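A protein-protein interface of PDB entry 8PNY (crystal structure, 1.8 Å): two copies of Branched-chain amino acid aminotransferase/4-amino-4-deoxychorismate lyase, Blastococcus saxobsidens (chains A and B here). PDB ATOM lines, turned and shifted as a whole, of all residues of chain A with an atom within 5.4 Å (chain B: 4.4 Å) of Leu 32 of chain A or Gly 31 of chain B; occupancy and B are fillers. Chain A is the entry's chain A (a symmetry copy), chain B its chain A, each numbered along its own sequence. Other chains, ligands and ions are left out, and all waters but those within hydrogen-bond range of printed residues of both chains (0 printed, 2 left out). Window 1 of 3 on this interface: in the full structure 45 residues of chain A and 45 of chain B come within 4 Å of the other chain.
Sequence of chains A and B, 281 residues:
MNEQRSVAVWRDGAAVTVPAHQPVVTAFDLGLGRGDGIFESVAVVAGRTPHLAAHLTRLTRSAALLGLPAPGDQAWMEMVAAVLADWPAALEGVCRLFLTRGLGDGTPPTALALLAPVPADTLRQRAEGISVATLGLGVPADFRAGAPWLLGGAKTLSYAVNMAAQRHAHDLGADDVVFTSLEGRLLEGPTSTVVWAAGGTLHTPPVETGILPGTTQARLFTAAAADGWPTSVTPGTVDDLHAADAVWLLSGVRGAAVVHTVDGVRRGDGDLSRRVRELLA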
ATOM      1  N   VAL A  25     -23.758   0.538   8.486  1.00  0.00           N
ATOM      2  CA  VAL A  25     -22.862  -0.523   7.967  1.00  0.00           C
ATOM      3  C   VAL A  25     -23.391  -0.996   6.605  1.00  0.00           C
ATOM      4  O   VAL A  25     -24.623  -1.176   6.461  1.00  0.00           O
ATOM      5  CB  VAL A  25     -22.760  -1.609   9.057  1.00  0.00           C
ATOM      6  CG1 VAL A  25     -22.704  -3.022   8.548  1.00  0.00           C
ATOM      7  CG2 VAL A  25     -21.587  -1.312   9.983  1.00  0.00           C
ATOM      8  N   THR A  26     -22.496  -1.126   5.619  1.00  0.00           N
ATOM      9  CA  THR A  26     -22.860  -1.609   4.266  1.00  0.00           C
ATOM     10  C   THR A  26     -22.954  -3.135   4.273  1.00  0.00           C
ATOM     11  O   THR A  26     -22.541  -3.781   5.266  1.00  0.00           O
ATOM     12  CB  THR A  26     -21.858  -1.228   3.182  1.00  0.00           C
ATOM     13  OG1 THR A  26     -20.695  -2.046   3.335  1.00  0.00           O
ATOM     14  CG2 THR A  26     -21.514   0.244   3.187  1.00  0.00           C
ATOM     15  N   ALA A  27     -23.485  -3.685   3.188  1.00  0.00           N
ATOM     16  CA  ALA A  27     -23.738  -5.132   3.035  1.00  0.00           C
ATOM     17  C   ALA A  27     -22.406  -5.893   3.106  1.00  0.00           C
ATOM     18  O   ALA A  27     -22.413  -7.035   3.593  1.00  0.00           O
ATOM     19  CB  ALA A  27     -24.506  -5.394   1.749  1.00  0.00           C
ATOM     20  N   ASP A  29     -19.662  -5.231   4.905  1.00  0.00           N
ATOM     21  CA  ASP A  29     -18.904  -5.170   6.184  1.00  0.00           C
ATOM     22  C   ASP A  29     -18.730  -6.594   6.732  1.00  0.00           C
ATOM     23  O   ASP A  29     -19.720  -7.338   6.862  1.00  0.00           O
ATOM     24  CB  ASP A  29     -19.561  -4.208   7.170  1.00  0.00           C
ATOM     25  CG  ASP A  29     -18.587  -3.793   8.250  1.00  0.00           C
ATOM     26  OD1 ASP A  29     -18.135  -4.641   8.973  1.00  0.00           O
ATOM     27  OD2 ASP A  29     -18.235  -2.652   8.270  1.00  0.00           O
ATOM     28  N   LEU A  30     -17.491  -6.974   7.027  1.00  0.00           N
ATOM     29  CA  LEU A  30     -17.180  -8.336   7.469  1.00  0.00           C
ATOM     30  C   LEU A  30     -17.696  -8.553   8.893  1.00  0.00           C
ATOM     31  O   LEU A  30     -17.893  -9.716   9.261  1.00  0.00           O
ATOM     32  CB  LEU A  30     -15.677  -8.554   7.387  1.00  0.00           C
ATOM     33  CG  LEU A  30     -15.118  -8.679   5.978  1.00  0.00           C
ATOM     34  CD1 LEU A  30     -13.613  -8.617   6.060  1.00  0.00           C
ATOM     35  CD2 LEU A  30     -15.562  -9.988   5.348  1.00  0.00           C
ATOM     36  N   GLY A  31     -18.042  -7.496   9.619  1.00  0.00           N
ATOM     37  CA  GLY A  31     -18.664  -7.653  10.941  1.00  0.00           C
ATOM     38  C   GLY A  31     -20.089  -8.127  10.771  1.00  0.00           C
ATOM     39  O   GLY A  31     -20.502  -8.986  11.547  1.00  0.00           O
ATOM     40  N   LEU A  32     -20.777  -7.682   9.710  1.00  0.00           N
ATOM     41  CA  LEU A  32     -22.112  -8.226   9.372  1.00  0.00           C
ATOM     42  C   LEU A  32     -22.030  -9.644   8.762  1.00  0.00           C
ATOM     43  O   LEU A  32     -22.698 -10.564   9.285  1.00  0.00           O
ATOM     44  CB  LEU A  32     -22.815  -7.221   8.462  1.00  0.00           C
ATOM     45  CG  LEU A  32     -24.150  -7.651   7.849  1.00  0.00           C
ATOM     46  CD1 LEU A  32     -25.184  -7.933   8.926  1.00  0.00           C
ATOM     47  CD2 LEU A  32     -24.670  -6.595   6.858  1.00  0.00           C
ATOM     48  N   GLY A  33     -21.358  -9.794   7.620  1.00  0.00           N
ATOM     49  CA  GLY A  33     -21.410 -11.038   6.831  1.00  0.00           C
ATOM     50  C   GLY A  33     -20.682 -12.184   7.487  1.00  0.00           C
ATOM     51  O   GLY A  33     -21.038 -13.315   7.223  1.00  0.00           O
ATOM     52  N   ARG A  34     -19.646 -11.928   8.280  1.00  0.00           N
ATOM     53  CA  ARG A  34     -18.781 -13.003   8.830  1.00  0.00           C
ATOM     54  C   ARG A  34     -18.696 -12.923  10.361  1.00  0.00           C
ATOM     55  O   ARG A  34     -18.042 -13.787  10.920  1.00  0.00           O
ATOM     56  CB  ARG A  34     -17.346 -12.916   8.287  1.00  0.00           C
ATOM     57  CG  ARG A  34     -17.227 -12.964   6.771  1.00  0.00           C
ATOM     58  CD  ARG A  34     -17.155 -14.371   6.195  1.00  0.00           C
ATOM     59  NE  ARG A  34     -17.694 -14.394   4.840  1.00  0.00           N
ATOM     60  CZ  ARG A  34     -17.001 -14.166   3.733  1.00  0.00           C
ATOM     61  NH1 ARG A  34     -15.695 -13.945   3.774  1.00  0.00           N
ATOM     62  NH2 ARG A  34     -17.635 -14.170   2.579  1.00  0.00           N
ATOM     63  N   GLY A  35     -19.274 -11.902  11.000  1.00  0.00           N
ATOM     64  CA  GLY A  35     -19.097 -11.731  12.463  1.00  0.00           C
ATOM     65  C   GLY A  35     -17.639 -11.529  12.834  1.00  0.00           C
ATOM     66  O   GLY A  35     -17.226 -11.894  13.932  1.00  0.00           O
ATOM     67  N   LEU A 157     -18.070 -10.420  17.532  1.00  0.00           N
ATOM     68  CA  LEU A 157     -19.393 -10.132  16.959  1.00  0.00           C
ATOM     69  C   LEU A 157     -20.054 -11.457  16.541  1.00  0.00           C
ATOM     70  O   LEU A 157     -21.187 -11.430  16.167  1.00  0.00           O
ATOM     71  CB  LEU A 157     -19.191  -9.114  15.834  1.00  0.00           C
ATOM     72  CG  LEU A 157     -18.762  -7.730  16.338  1.00  0.00           C
ATOM     73  CD1 LEU A 157     -18.640  -6.726  15.222  1.00  0.00           C
ATOM     74  CD2 LEU A 157     -19.750  -7.227  17.360  1.00  0.00           C
ATOM     75  N   VAL B  25     -27.512  -1.472   7.084  1.00  0.00           N
ATOM     76  CA  VAL B  25     -27.812  -2.081   8.402  1.00  0.00           C
ATOM     77  C   VAL B  25     -27.476  -1.066   9.504  1.00  0.00           C
ATOM     78  O   VAL B  25     -26.417  -0.402   9.417  1.00  0.00           O
ATOM     79  CB  VAL B  25     -27.049  -3.420   8.472  1.00  0.00           C
ATOM     80  CG1 VAL B  25     -26.479  -3.760   9.820  1.00  0.00           C
ATOM     81  CG2 VAL B  25     -27.925  -4.549   7.944  1.00  0.00           C
ATOM     82  N   ASP B  29     -28.704  -3.838  14.557  1.00  0.00           N
ATOM     83  CA  ASP B  29     -29.030  -5.111  13.858  1.00  0.00           C
ATOM     84  C   ASP B  29     -28.284  -6.265  14.544  1.00  0.00           C
ATOM     85  O   ASP B  29     -27.056  -6.189  14.734  1.00  0.00           O
ATOM     86  CB  ASP B  29     -28.754  -5.005  12.362  1.00  0.00           C
ATOM     87  CG  ASP B  29     -29.491  -6.083  11.599  1.00  0.00           C
ATOM     88  OD1 ASP B  29     -29.231  -7.233  11.832  1.00  0.00           O
ATOM     89  OD2 ASP B  29     -30.373  -5.740  10.869  1.00  0.00           O
ATOM     90  N   LEU B  30     -29.016  -7.305  14.930  1.00  0.00           N
ATOM     91  CA  LEU B  30     -28.441  -8.428  15.676  1.00  0.00           C
ATOM     92  C   LEU B  30     -27.549  -9.263  14.757  1.00  0.00           C
ATOM     93  O   LEU B  30     -26.684  -9.971  15.283  1.00  0.00           O
ATOM     94  CB  LEU B  30     -29.567  -9.264  16.263  1.00  0.00           C
ATOM     95  CG  LEU B  30     -30.310  -8.623  17.425  1.00  0.00           C
ATOM     96  CD1 LEU B  30     -31.544  -9.444  17.705  1.00  0.00           C
ATOM     97  CD2 LEU B  30     -29.419  -8.566  18.653  1.00  0.00           C
ATOM     98  N   GLY B  31     -27.641  -9.092  13.442  1.00  0.00           N
ATOM     99  CA  GLY B  31     -26.720  -9.772  12.521  1.00  0.00           C
ATOM    100  C   GLY B  31     -25.356  -9.128  12.609  1.00  0.00           C
ATOM    101  O   GLY B  31     -24.374  -9.865  12.597  1.00  0.00           O
ATOM    102  N   LEU B  32     -25.299  -7.806  12.825  1.00  0.00           N
ATOM    103  CA  LEU B  32     -24.013  -7.123  13.096  1.00  0.00           C
ATOM    104  C   LEU B  32     -23.488  -7.408  14.522  1.00  0.00           C
ATOM    105  O   LEU B  32     -22.329  -7.862  14.656  1.00  0.00           O
ATOM    106  CB  LEU B  32     -24.200  -5.634  12.813  1.00  0.00           C
ATOM    107  CG  LEU B  32     -23.044  -4.703  13.186  1.00  0.00           C
ATOM    108  CD1 LEU B  32     -21.785  -5.053  12.411  1.00  0.00           C
ATOM    109  CD2 LEU B  32     -23.427  -3.229  12.966  1.00  0.00           C
ATOM    110  N   GLY B  33     -24.242  -7.027  15.553  1.00  0.00           N
ATOM    111  CA  GLY B  33     -23.744  -7.033  16.939  1.00  0.00           C
ATOM    112  C   GLY B  33     -23.566  -8.423  17.498  1.00  0.00           C
ATOM    113  O   GLY B  33     -22.749  -8.585  18.381  1.00  0.00           O
ATOM    114  N   GLY B  35     -23.974 -11.509  15.326  1.00  0.00           N
ATOM    115  CA  GLY B  35     -23.840 -12.553  14.282  1.00  0.00           C
ATOM    116  C   GLY B  35     -25.036 -13.486  14.260  1.00  0.00           C
ATOM    117  O   GLY B  35     -24.903 -14.651  13.895  1.00  0.00           O
ATOM    118  N   ASP B  36     -26.212 -12.958  14.596  1.00  0.00           N
ATOM    119  CA  ASP B  36     -27.465 -13.721  14.782  1.00  0.00           C
ATOM    120  C   ASP B  36     -28.280 -13.655  13.489  1.00  0.00           C
ATOM    121  O   ASP B  36     -29.172 -12.812  13.350  1.00  0.00           O
ATOM    122  CB  ASP B  36     -28.228 -13.217  16.003  1.00  0.00           C
ATOM    123  CG  ASP B  36     -29.276 -14.205  16.493  1.00  0.00           C
ATOM    124  OD1 ASP B  36     -29.378 -15.343  15.911  1.00  0.00           O
ATOM    125  OD2 ASP B  36     -30.043 -13.792  17.382  1.00  0.00           O
ATOM    126  N   PHE B  98     -28.456 -12.788   2.958  1.00  0.00           N
ATOM    127  CA  PHE B  98     -28.321 -12.636   4.424  1.00  0.00           C
ATOM    128  C   PHE B  98     -29.698 -12.421   5.010  1.00  0.00           C
ATOM    129  O   PHE B  98     -30.460 -11.595   4.454  1.00  0.00           O
ATOM    130  CB  PHE B  98     -27.575 -11.372   4.817  1.00  0.00           C
ATOM    131  CG  PHE B  98     -26.115 -11.339   4.489  1.00  0.00           C
ATOM    132  CD1 PHE B  98     -25.449 -12.455   4.017  1.00  0.00           C
ATOM    133  CD2 PHE B  98     -25.406 -10.167   4.699  1.00  0.00           C
ATOM    134  CE1 PHE B  98     -24.088 -12.395   3.736  1.00  0.00           C
ATOM    135  CE2 PHE B  98     -24.056 -10.102   4.403  1.00  0.00           C
ATOM    136  CZ  PHE B  98     -23.392 -11.219   3.931  1.00  0.00           C
ATOM    137  N   THR B 100     -31.034 -11.678   8.965  1.00  0.00           N
ATOM    138  CA  THR B 100     -30.653 -11.395  10.365  1.00  0.00           C
ATOM    139  C   THR B 100     -31.913 -11.323  11.222  1.00  0.00           C
ATOM    140  O   THR B 100     -33.041 -11.095  10.666  1.00  0.00           O
ATOM    141  CB  THR B 100     -29.816 -10.123  10.500  1.00  0.00           C
ATOM    142  OG1 THR B 100     -30.728  -9.033  10.601  1.00  0.00           O
ATOM    143  CG2 THR B 100     -28.900  -9.885   9.322  1.00  0.00           C
ATOM    144  N   LEU B 112     -31.126  -9.302   2.886  1.00  0.00           N
ATOM    145  CA  LEU B 112     -30.297  -8.584   1.881  1.00  0.00           C
ATOM    146  C   LEU B 112     -29.825  -9.592   0.847  1.00  0.00           C
ATOM    147  O   LEU B 112     -29.638 -10.754   1.215  1.00  0.00           O
ATOM    148  CB  LEU B 112     -29.047  -7.978   2.531  1.00  0.00           C
ATOM    149  CG  LEU B 112     -29.274  -7.214   3.829  1.00  0.00           C
ATOM    150  CD1 LEU B 112     -28.019  -7.198   4.695  1.00  0.00           C
ATOM    151  CD2 LEU B 112     -29.713  -5.803   3.499  1.00  0.00           C
ATOM    152  N   LEU B 157     -24.087 -16.048  10.258  1.00  0.00           N
ATOM    153  CA  LEU B 157     -23.308 -14.811  10.101  1.00  0.00           C
ATOM    154  C   LEU B 157     -22.179 -14.798  11.147  1.00  0.00           C
ATOM    155  O   LEU B 157     -21.367 -13.924  11.089  1.00  0.00           O
ATOM    156  CB  LEU B 157     -24.290 -13.641  10.178  1.00  0.00           C
ATOM    157  CG  LEU B 157     -25.241 -13.566   8.976  1.00  0.00           C
ATOM    158  CD1 LEU B 157     -26.149 -12.366   9.038  1.00  0.00           C
ATOM    159  CD2 LEU B 157     -24.446 -13.528   7.695  1.00  0.00           C
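Of the printed residues of chain B, Leu 32 of chain A touches Val 25 (3.995 Å), Gly 31 (3.8 Å), Leu 32 (3.9 Å) and Leu 157 (3.6 Å). Printed residues of chain B within 4 Å of Leu 157 of chain A: Leu 32, Gly 33 and Gly 35. Gly 31 of chain B touches just one residue of chain A: Leu 32 (3.8 Å). Of the printed residues of chain A, Leu 32 of chain B touches Val 25, Gly 31, Leu 32 and Leu 157. Printed residues of chain A within 4 Å of Gly 35 of chain B: Leu 157 (2.9 Å). Of the printed residues of chain A, Phe 98 of chain B touches Ala 27 and Gly 33. Of the printed residues of chain A, Leu 157 of chain B touches Leu 32 (3.6 Å), Gly 33 (3.4 Å), Arg 34 (2.9 Å) and Gly 35 (2.9 Å). The nearest printed residue of chain B that does not touch Leu 32 of chain A is Leu 112 of chain B (4.03 Å).
Val 25 of chain B touches its own counterpart, Val 25 of chain A. Gly 31 of chain A touches Leu 32 of chain B, and with the chains exchanged Leu 32 of chain A touches Gly 31 of chain B. Leu 32 of chain A touches Leu 157 of chain B, and with the chains exchanged Leu 157 of chain A touches Leu 32 of chain B. Gly 33 of chain A touches Leu 157 of chain B, and with the chains exchanged Leu 157 of chain A touches Gly 33 of chain B. Of the 15 pairs that touch across the chains among the printed residues, 12 have their exchanged pair printed and touching as well.
OD1 of Asp 29 of chain B lies within hydrogen-bond range of N of Gly 31 of chain B. O of Leu 30 of chain B is in hydrogen-bond range of N of Gly 35 of chain B. The backbone NH of Leu 112 of chain B is in hydrogen-bond range of the backbone carbonyl oxygen of Phe 98 of chain B (2.9 Å). The side-chain carboxylate (OD1) of Asp 29 of chain A is in hydrogen-bond range of the backbone NH (N) of Gly 31 of chain A, 2.9 Å away. The backbone carbonyl oxygen (O) of Leu 30 of chain A sits at hydrogen-bond distance from the backbone NH (N) of Gly 35 of chain A (3.1 Å).
Among the printed residues, merely in contact across the chains: Leu 157 of chain A with Gly 33 of chain B, Gly 33 of chain A with Leu 157 of chain B, Gly 33 of chain A with Phe 98 of chain B, Ala 27 of chain A with Phe 98 of chain B, Leu 32 of chain A with Leu 157 of chain B, Leu 157 of chain A with Leu 32 of chain B, Leu 32 of chain A with Gly 31 of chain B, Gly 31 of chain A with Leu 32 of chain B, Leu 32 of chain A with Leu 32 of chain B, Val 25 of chain A with Leu 32 of chain B and Leu 32 of chain A with Val 25 of chain B.
N of Val 25 of chain B sits at hydrogen-bond distance from O of Val 25 of chain A. N of Gly 35 of chain B lies within hydrogen-bond range of O of Leu 157 of chain A (2.9 Å). N of Gly 35 of chain A is in hydrogen-bond range of O of Leu 157 of chain B. O of Leu 157 of chain B sits close to O of Arg 34 of chain A (3.3 Å).
Of the 12 printed residues of chain B, 7 touch a printed residue of chain A. Printed residues of chain B that touch a printed residue of chain A: Val 25, Gly 31, Leu 32, Gly 33, Gly 35, Phe 98 and Leu 157. Hydrophobic or aromatic side chains of chain B that line the printed part of chain A: Val 25, Leu 32, Phe 98 and Leu 157. Among the printed residues, no Asp or Glu carboxylate lies within 4 Å of a Lys or Arg side-chain nitrogen of the other chain.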
